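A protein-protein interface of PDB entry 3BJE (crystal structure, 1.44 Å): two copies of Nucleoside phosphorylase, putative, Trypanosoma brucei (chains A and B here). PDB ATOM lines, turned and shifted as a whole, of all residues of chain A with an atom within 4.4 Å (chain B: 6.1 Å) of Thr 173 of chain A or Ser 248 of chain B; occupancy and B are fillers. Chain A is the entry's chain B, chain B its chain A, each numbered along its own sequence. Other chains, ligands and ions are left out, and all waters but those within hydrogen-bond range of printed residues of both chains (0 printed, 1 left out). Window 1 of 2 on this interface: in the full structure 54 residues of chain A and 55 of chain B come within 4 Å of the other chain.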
ATOM      1  N   VAL A  97      34.767  19.096   9.353  1.00  0.00           N
ATOM      2  CA  VAL A  97      33.597  19.023  10.231  1.00  0.00           C
ATOM      3  C   VAL A  97      32.261  19.300   9.517  1.00  0.00           C
ATOM      4  O   VAL A  97      31.196  18.828   9.929  1.00  0.00           O
ATOM      5  CB  VAL A  97      33.767  19.949  11.438  1.00  0.00           C
ATOM      6  CG1 VAL A  97      34.864  19.390  12.375  1.00  0.00           C
ATOM      7  CG2 VAL A  97      34.114  21.364  10.997  1.00  0.00           C
ATOM      8  N   ASP A  98      32.340  20.066   8.442  1.00  0.00           N
ATOM      9  CA  ASP A  98      31.197  20.285   7.569  1.00  0.00           C
ATOM     10  C   ASP A  98      30.752  18.994   6.913  1.00  0.00           C
ATOM     11  O   ASP A  98      29.550  18.701   6.865  1.00  0.00           O
ATOM     12  CB  ASP A  98      31.502  21.361   6.514  1.00  0.00           C
ATOM     13  CG  ASP A  98      32.672  21.004   5.601  1.00  0.00           C
ATOM     14  OD1 ASP A  98      33.639  20.365   6.042  1.00  0.00           O
ATOM     15  OD2 ASP A  98      32.657  21.418   4.424  1.00  0.00           O
ATOM     16  N   GLU A 101      29.087  16.903   9.513  1.00  0.00           N
ATOM     17  CA  GLU A 101      27.723  17.386   9.763  1.00  0.00           C
ATOM     18  C   GLU A 101      26.776  16.764   8.732  1.00  0.00           C
ATOM     19  O   GLU A 101      25.684  16.271   9.062  1.00  0.00           O
ATOM     20  CB  GLU A 101      27.675  18.920   9.704  1.00  0.00           C
ATOM     21  CG  GLU A 101      26.388  19.538  10.207  1.00  0.00           C
ATOM     22  CD  GLU A 101      25.447  20.053   9.126  1.00  0.00           C
ATOM     23  OE1 GLU A 101      25.630  19.706   7.933  1.00  0.00           O
ATOM     24  OE2 GLU A 101      24.498  20.798   9.477  1.00  0.00           O
ATOM     25  N   ASP A 171      36.917  24.897  14.708  1.00  0.00           N
ATOM     26  CA  ASP A 171      35.905  25.115  13.681  1.00  0.00           C
ATOM     27  C   ASP A 171      34.688  25.779  14.301  1.00  0.00           C
ATOM     28  O   ASP A 171      34.673  26.023  15.507  1.00  0.00           O
ATOM     29  CB  ASP A 171      35.490  23.778  13.100  1.00  0.00           C
ATOM     30  CG  ASP A 171      34.855  22.895  14.143  1.00  0.00           C
ATOM     31  OD1 ASP A 171      35.593  22.438  15.048  1.00  0.00           O
ATOM     32  OD2 ASP A 171      33.613  22.749  14.113  1.00  0.00           O
ATOM     33  N   ASN A 172      33.656  26.039  13.484  1.00  0.00           N
ATOM     34  CA  ASN A 172      32.422  26.576  14.027  1.00  0.00           C
ATOM     35  C   ASN A 172      31.169  25.790  13.672  1.00  0.00           C
ATOM     36  O   ASN A 172      30.067  26.247  13.937  1.00  0.00           O
ATOM     37  CB  ASN A 172      32.223  28.072  13.641  1.00  0.00           C
ATOM     38  CG  ASN A 172      31.562  28.265  12.289  1.00  0.00           C
ATOM     39  OD1 ASN A 172      31.531  27.367  11.447  1.00  0.00           O
ATOM     40  ND2 ASN A 172      31.067  29.494  12.057  1.00  0.00           N
ATOM     41  N   THR A 173      31.304  24.581  13.127  1.00  0.00           N
ATOM     42  CA  THR A 173      30.148  23.837  12.645  1.00  0.00           C
ATOM     43  C   THR A 173      29.149  23.609  13.754  1.00  0.00           C
ATOM     44  O   THR A 173      27.927  23.816  13.561  1.00  0.00           O
ATOM     45  CB  THR A 173      30.618  22.536  11.962  1.00  0.00           C
ATOM     46  OG1 THR A 173      31.321  22.901  10.768  1.00  0.00           O
ATOM     47  CG2 THR A 173      29.419  21.621  11.645  1.00  0.00           C
ATOM     48  N   SER A 174      29.641  23.244  14.938  1.00  0.00           N
ATOM     49  CA  SER A 174      28.716  22.947  16.031  1.00  0.00           C
ATOM     50  C   SER A 174      28.140  24.211  16.671  1.00  0.00           C
ATOM     51  O   SER A 174      27.231  24.126  17.503  1.00  0.00           O
ATOM     52  CB  SER A 174      29.376  22.061  17.090  1.00  0.00           C
ATOM     53  OG  SER A 174      29.895  20.845  16.544  1.00  0.00           O
ATOM     54  N   LEU A 175      28.637  25.396  16.294  1.00  0.00           N
ATOM     55  CA  LEU A 175      27.995  26.619  16.788  1.00  0.00           C
ATOM     56  C   LEU A 175      26.589  26.746  16.279  1.00  0.00           C
ATOM     57  O   LEU A 175      25.804  27.504  16.856  1.00  0.00           O
ATOM     58  CB  LEU A 175      28.779  27.889  16.443  1.00  0.00           C
ATOM     59  CG  LEU A 175      30.144  28.081  17.101  1.00  0.00           C
ATOM     60  CD1 LEU A 175      30.640  29.508  16.901  1.00  0.00           C
ATOM     61  CD2 LEU A 175      30.166  27.729  18.590  1.00  0.00           C
ATOM     62  N   TYR A 176      26.285  26.047  15.192  1.00  0.00           N
ATOM     63  CA  TYR A 176      24.935  26.025  14.609  1.00  0.00           C
ATOM     64  C   TYR A 176      23.984  25.064  15.343  1.00  0.00           C
ATOM     65  O   TYR A 176      22.783  24.999  15.035  1.00  0.00           O
ATOM     66  CB  TYR A 176      25.015  25.789  13.093  1.00  0.00           C
ATOM     67  CG  TYR A 176      25.585  27.023  12.456  1.00  0.00           C
ATOM     68  CD1 TYR A 176      24.764  28.106  12.172  1.00  0.00           C
ATOM     69  CD2 TYR A 176      26.949  27.184  12.286  1.00  0.00           C
ATOM     70  CE1 TYR A 176      25.277  29.273  11.669  1.00  0.00           C
ATOM     71  CE2 TYR A 176      27.476  28.373  11.780  1.00  0.00           C
ATOM     72  CZ  TYR A 176      26.627  29.419  11.486  1.00  0.00           C
ATOM     73  OH  TYR A 176      27.125  30.608  11.019  1.00  0.00           O
ATOM     74  N   TYR A 177      24.536  24.336  16.317  1.00  0.00           N
ATOM     75  CA  TYR A 177      23.833  23.360  17.132  1.00  0.00           C
ATOM     76  C   TYR A 177      23.970  23.767  18.609  1.00  0.00           C
ATOM     77  O   TYR A 177      24.136  22.906  19.491  1.00  0.00           O
ATOM     78  CB  TYR A 177      24.387  21.967  16.893  1.00  0.00           C
ATOM     79  CG  TYR A 177      24.151  21.453  15.498  1.00  0.00           C
ATOM     80  CD1 TYR A 177      23.143  20.527  15.238  1.00  0.00           C
ATOM     81  CD2 TYR A 177      24.924  21.899  14.411  1.00  0.00           C
ATOM     82  CE1 TYR A 177      22.904  20.054  13.947  1.00  0.00           C
ATOM     83  CE2 TYR A 177      24.682  21.435  13.120  1.00  0.00           C
ATOM     84  CZ  TYR A 177      23.668  20.502  12.893  1.00  0.00           C
ATOM     85  OH  TYR A 177      23.388  19.970  11.635  1.00  0.00           O
ATOM     86  N   VAL B  97      34.468  25.212   2.806  1.00  0.00           N
ATOM     87  CA  VAL B  97      35.465  26.276   2.873  1.00  0.00           C
ATOM     88  C   VAL B  97      36.813  25.798   3.410  1.00  0.00           C
ATOM     89  O   VAL B  97      37.856  26.365   3.101  1.00  0.00           O
ATOM     90  CB  VAL B  97      34.974  27.483   3.723  1.00  0.00           C
ATOM     91  CG1 VAL B  97      33.871  28.267   2.971  1.00  0.00           C
ATOM     92  CG2 VAL B  97      34.535  27.042   5.130  1.00  0.00           C
ATOM     93  N   MET B 170      29.352  32.549   6.927  1.00  0.00           N
ATOM     94  CA  MET B 170      28.771  31.993   8.150  1.00  0.00           C
ATOM     95  C   MET B 170      29.686  30.913   8.755  1.00  0.00           C
ATOM     96  O   MET B 170      29.497  30.494   9.890  1.00  0.00           O
ATOM     97  CB  MET B 170      27.386  31.427   7.876  1.00  0.00           C
ATOM     98  CG  MET B 170      26.460  32.419   7.169  1.00  0.00           C
ATOM     99  SD  MET B 170      24.760  31.847   6.978  1.00  0.00           S
ATOM    100  CE  MET B 170      25.027  30.423   5.897  1.00  0.00           C
ATOM    101  N   ASP B 171      30.608  30.425   7.938  1.00  0.00           N
ATOM    102  CA  ASP B 171      31.684  29.565   8.359  1.00  0.00           C
ATOM    103  C   ASP B 171      32.692  30.396   9.160  1.00  0.00           C
ATOM    104  O   ASP B 171      32.508  31.612   9.330  1.00  0.00           O
ATOM    105  CB  ASP B 171      32.364  29.018   7.119  1.00  0.00           C
ATOM    106  CG  ASP B 171      32.974  30.129   6.280  1.00  0.00           C
ATOM    107  OD1 ASP B 171      32.222  30.933   5.663  1.00  0.00           O
ATOM    108  OD2 ASP B 171      34.229  30.237   6.286  1.00  0.00           O
ATOM    109  N   ASN B 172      33.779  29.762   9.626  1.00  0.00           N
ATOM    110  CA  ASN B 172      34.842  30.491  10.334  1.00  0.00           C
ATOM    111  C   ASN B 172      36.240  30.326   9.755  1.00  0.00           C
ATOM    112  O   ASN B 172      37.216  30.758  10.342  1.00  0.00           O
ATOM    113  CB  ASN B 172      34.848  30.208  11.848  1.00  0.00           C
ATOM    114  CG  ASN B 172      35.661  28.986  12.253  1.00  0.00           C
ATOM    115  OD1 ASN B 172      35.962  28.128  11.423  1.00  0.00           O
ATOM    116  ND2 ASN B 172      35.991  28.886  13.565  1.00  0.00           N
ATOM    117  N   THR B 246      27.580  31.587   2.803  1.00  0.00           N
ATOM    118  CA  THR B 246      28.299  30.334   2.858  1.00  0.00           C
ATOM    119  C   THR B 246      28.291  29.725   4.267  1.00  0.00           C
ATOM    120  O   THR B 246      28.593  30.385   5.256  1.00  0.00           O
ATOM    121  CB  THR B 246      29.754  30.517   2.398  1.00  0.00           C
ATOM    122  OG1 THR B 246      29.769  31.010   1.053  1.00  0.00           O
ATOM    123  CG2 THR B 246      30.585  29.198   2.488  1.00  0.00           C
ATOM    124  N   ALA B 247      27.983  28.428   4.297  1.00  0.00           N
ATOM    125  CA  ALA B 247      27.741  27.681   5.514  1.00  0.00           C
ATOM    126  C   ALA B 247      28.842  26.671   5.790  1.00  0.00           C
ATOM    127  O   ALA B 247      29.537  26.204   4.867  1.00  0.00           O
ATOM    128  CB  ALA B 247      26.416  26.920   5.384  1.00  0.00           C
ATOM    129  N   SER B 248      28.979  26.302   7.074  1.00  0.00           N
ATOM    130  CA  SER B 248      29.954  25.293   7.542  1.00  0.00           C
ATOM    131  C   SER B 248      29.322  23.900   7.724  1.00  0.00           C
ATOM    132  O   SER B 248      29.747  23.087   8.539  1.00  0.00           O
ATOM    133  CB  SER B 248      30.628  25.771   8.815  1.00  0.00           C
ATOM    134  OG  SER B 248      29.687  26.128   9.819  1.00  0.00           O
ATOM    135  N   GLY B 249      28.282  23.667   6.910  1.00  0.00           N
ATOM    136  CA  GLY B 249      27.526  22.409   6.872  1.00  0.00           C
ATOM    137  C   GLY B 249      26.380  22.556   5.899  1.00  0.00           C
ATOM    138  O   GLY B 249      26.268  23.564   5.210  1.00  0.00           O
ATOM    139  N   PHE B 250      25.547  21.528   5.831  1.00  0.00           N
ATOM    140  CA  PHE B 250      24.427  21.475   4.900  1.00  0.00           C
ATOM    141  C   PHE B 250      23.043  21.533   5.562  1.00  0.00           C
ATOM    142  O   PHE B 250      22.082  21.984   4.955  1.00  0.00           O
ATOM    143  CB  PHE B 250      24.524  20.178   4.103  1.00  0.00           C
ATOM    144  CG  PHE B 250      23.540  20.076   2.978  1.00  0.00           C
ATOM    145  CD1 PHE B 250      23.851  20.604   1.739  1.00  0.00           C
ATOM    146  CD2 PHE B 250      22.330  19.444   3.136  1.00  0.00           C
ATOM    147  CE1 PHE B 250      22.974  20.511   0.679  1.00  0.00           C
ATOM    148  CE2 PHE B 250      21.446  19.322   2.075  1.00  0.00           C
ATOM    149  CZ  PHE B 250      21.770  19.864   0.848  1.00  0.00           C
ATOM    150  N   CYS B 253      23.318  23.717   9.805  1.00  0.00           N
ATOM    151  CA  CYS B 253      24.164  24.838   9.373  1.00  0.00           C
ATOM    152  C   CYS B 253      23.592  25.728   8.303  1.00  0.00           C
ATOM    153  O   CYS B 253      24.099  26.832   8.099  1.00  0.00           O
ATOM    154  CB  CYS B 253      25.498  24.297   8.914  1.00  0.00           C
ATOM    155  SG  CYS B 253      26.489  23.580  10.262  1.00  0.00           S
ATOM    156  N   GLU B 292      25.346  28.231  -0.024  1.00  0.00           N
ATOM    157  CA  GLU B 292      26.152  27.067  -0.391  1.00  0.00           C
ATOM    158  C   GLU B 292      27.331  26.934   0.599  1.00  0.00           C
ATOM    159  O   GLU B 292      27.278  27.496   1.723  1.00  0.00           O
ATOM    160  CB  GLU B 292      26.578  27.120  -1.872  1.00  0.00           C
ATOM    161  CG  GLU B 292      27.153  28.459  -2.363  1.00  0.00           C
ATOM    162  CD  GLU B 292      28.516  28.719  -1.776  1.00  0.00           C
ATOM    163  OE1 GLU B 292      29.499  28.223  -2.370  1.00  0.00           O
ATOM    164  OE2 GLU B 292      28.574  29.392  -0.719  1.00  0.00           O
ATOM    165  N   MET B 293      28.388  26.212   0.226  1.00  0.00           N
ATOM    166  CA  MET B 293      29.410  25.832   1.217  1.00  0.00           C
ATOM    167  C   MET B 293      30.869  26.233   0.931  1.00  0.00           C
ATOM    168  O   MET B 293      31.747  25.862   1.702  1.00  0.00           O
ATOM    169  CB  MET B 293      29.341  24.319   1.457  1.00  0.00           C
ATOM    170  CG  MET B 293      28.019  23.878   2.070  1.00  0.00           C
ATOM    171  SD  MET B 293      27.850  22.106   2.351  1.00  0.00           S
ATOM    172  CE  MET B 293      29.173  21.832   3.578  1.00  0.00           C
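The backbone carbonyl oxygen of Met 170 of chain B is in hydrogen-bond range of the side-chain amide nitrogen of Asn 172 of chain A, 2.9 Å away. The side-chain hydroxyl (OH) of Tyr 176 of chain A lies within hydrogen-bond range of the backbone carbonyl oxygen (O) of Met 170 of chain B, 2.6 Å away. The side-chain hydroxyl of Ser 248 of chain B sits at hydrogen-bond distance from the side-chain amide oxygen of Asn 172 of chain A. O of Ser 248 of chain B lies within hydrogen-bond range of OG1 of Thr 173 of chain A (2.7 Å). The side-chain carboxylate of Glu 101 of chain A is in hydrogen-bond range of the backbone NH of Phe 250 of chain B. N of Cys 253 of chain B sits at hydrogen-bond distance from OE2 of Glu 101 of chain A, 3.2 Å away. SG of Cys 253 of chain B sits at hydrogen-bond distance from O of Thr 173 of chain A, at 3.6 Å.
Ser 248 of chain B touches Asp 98 of chain A. CB of Asp 98 of chain A touches N of Gly 249 of chain B (3.98 Å). Asp 98 of chain A touches Met 293 of chain B. OE1 of Glu 101 of chain A touches CA of Gly 249 of chain B (3.5 Å). Asp 171 of chain A touches Asn 172 of chain B (C to ND2, 3.4 Å). Asn 172 of chain A touches Asp 171 of chain B (ND2 to C, 3.4 Å). Asn 172 of chain B touches Asn 172 of chain A. Ser 248 of chain B touches Tyr 176 of chain A. CB of Tyr 176 of chain A touches SG of Cys 253 of chain B, 3.9 Å away.
Asp 171 of chain A touches Asn 172 of chain B, and with the chains exchanged Asn 172 of chain A touches Asp 171 of chain B. Asn 172 of chain A touches its own counterpart, Asn 172 of chain B. Positions printed for both chains: 97, 171 and 172. Of the 16 pairs that touch across the chains among the printed residues, 3 have their exchanged pair printed and touching as well.
Printed residues of chain B within 4 Å of Thr 173 of chain A: Ser 248 and Cys 253. Of the printed residues of chain A, Ser 248 of chain B touches Asp 98 (3.2 Å), Asn 172 (2.8 Å), Thr 173 (2.7 Å) and Tyr 176 (3.7 Å). Of the printed residues of chain B, Tyr 176 of chain A touches Met 170, Ser 248 and Cys 253. Of the printed residues of chain A, Met 170 of chain B touches Asn 172 and Tyr 176. Of the printed residues of chain A, Cys 253 of chain B touches Glu 101 (3.2 Å), Thr 173 (3.6 Å) and Tyr 176 (3.9 Å). Of the printed residues of chain B, Asn 172 of chain A touches Met 170 (2.9 Å), Asp 171 (3.4 Å), Asn 172 (3.7 Å) and Ser 248 (2.8 Å).
Hydrophobic or aromatic side chains of chain A that line the printed part of chain B: Tyr 176. Of the 12 printed residues of chain B, 8 touch a printed residue of chain A. Hydrophobic or aromatic side chains of chain B within 4 Å of the printed part of chain A: Met 170 and Met 293. Among the printed residues, 16 pairs touch across the chains.
The backbone NH (N) of Val 97 of chain B sits at hydrogen-bond distance from the backbone carbonyl oxygen (O) of Met 293 of chain B (3.0 Å). O of Thr 246 of chain B lies within hydrogen-bond range of N of Met 170 of chain B, 2.8 Å away. N of Asp 171 of chain B sits at hydrogen-bond distance from O of Thr 246 of chain B (3.4 Å). The backbone carbonyl oxygen of Ser 248 of chain B sits at hydrogen-bond distance from the side-chain sulfur of Cys 253 of chain B (3.7 Å). OH of Tyr 177 of chain A sits at hydrogen-bond distance from OE2 of Glu 101 of chain A (2.6 Å). The side-chain carboxylate (OD2) of Asp 171 of chain A lies within hydrogen-bond range of the backbone NH (N) of Thr 173 of chain A, at 3.1 Å.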
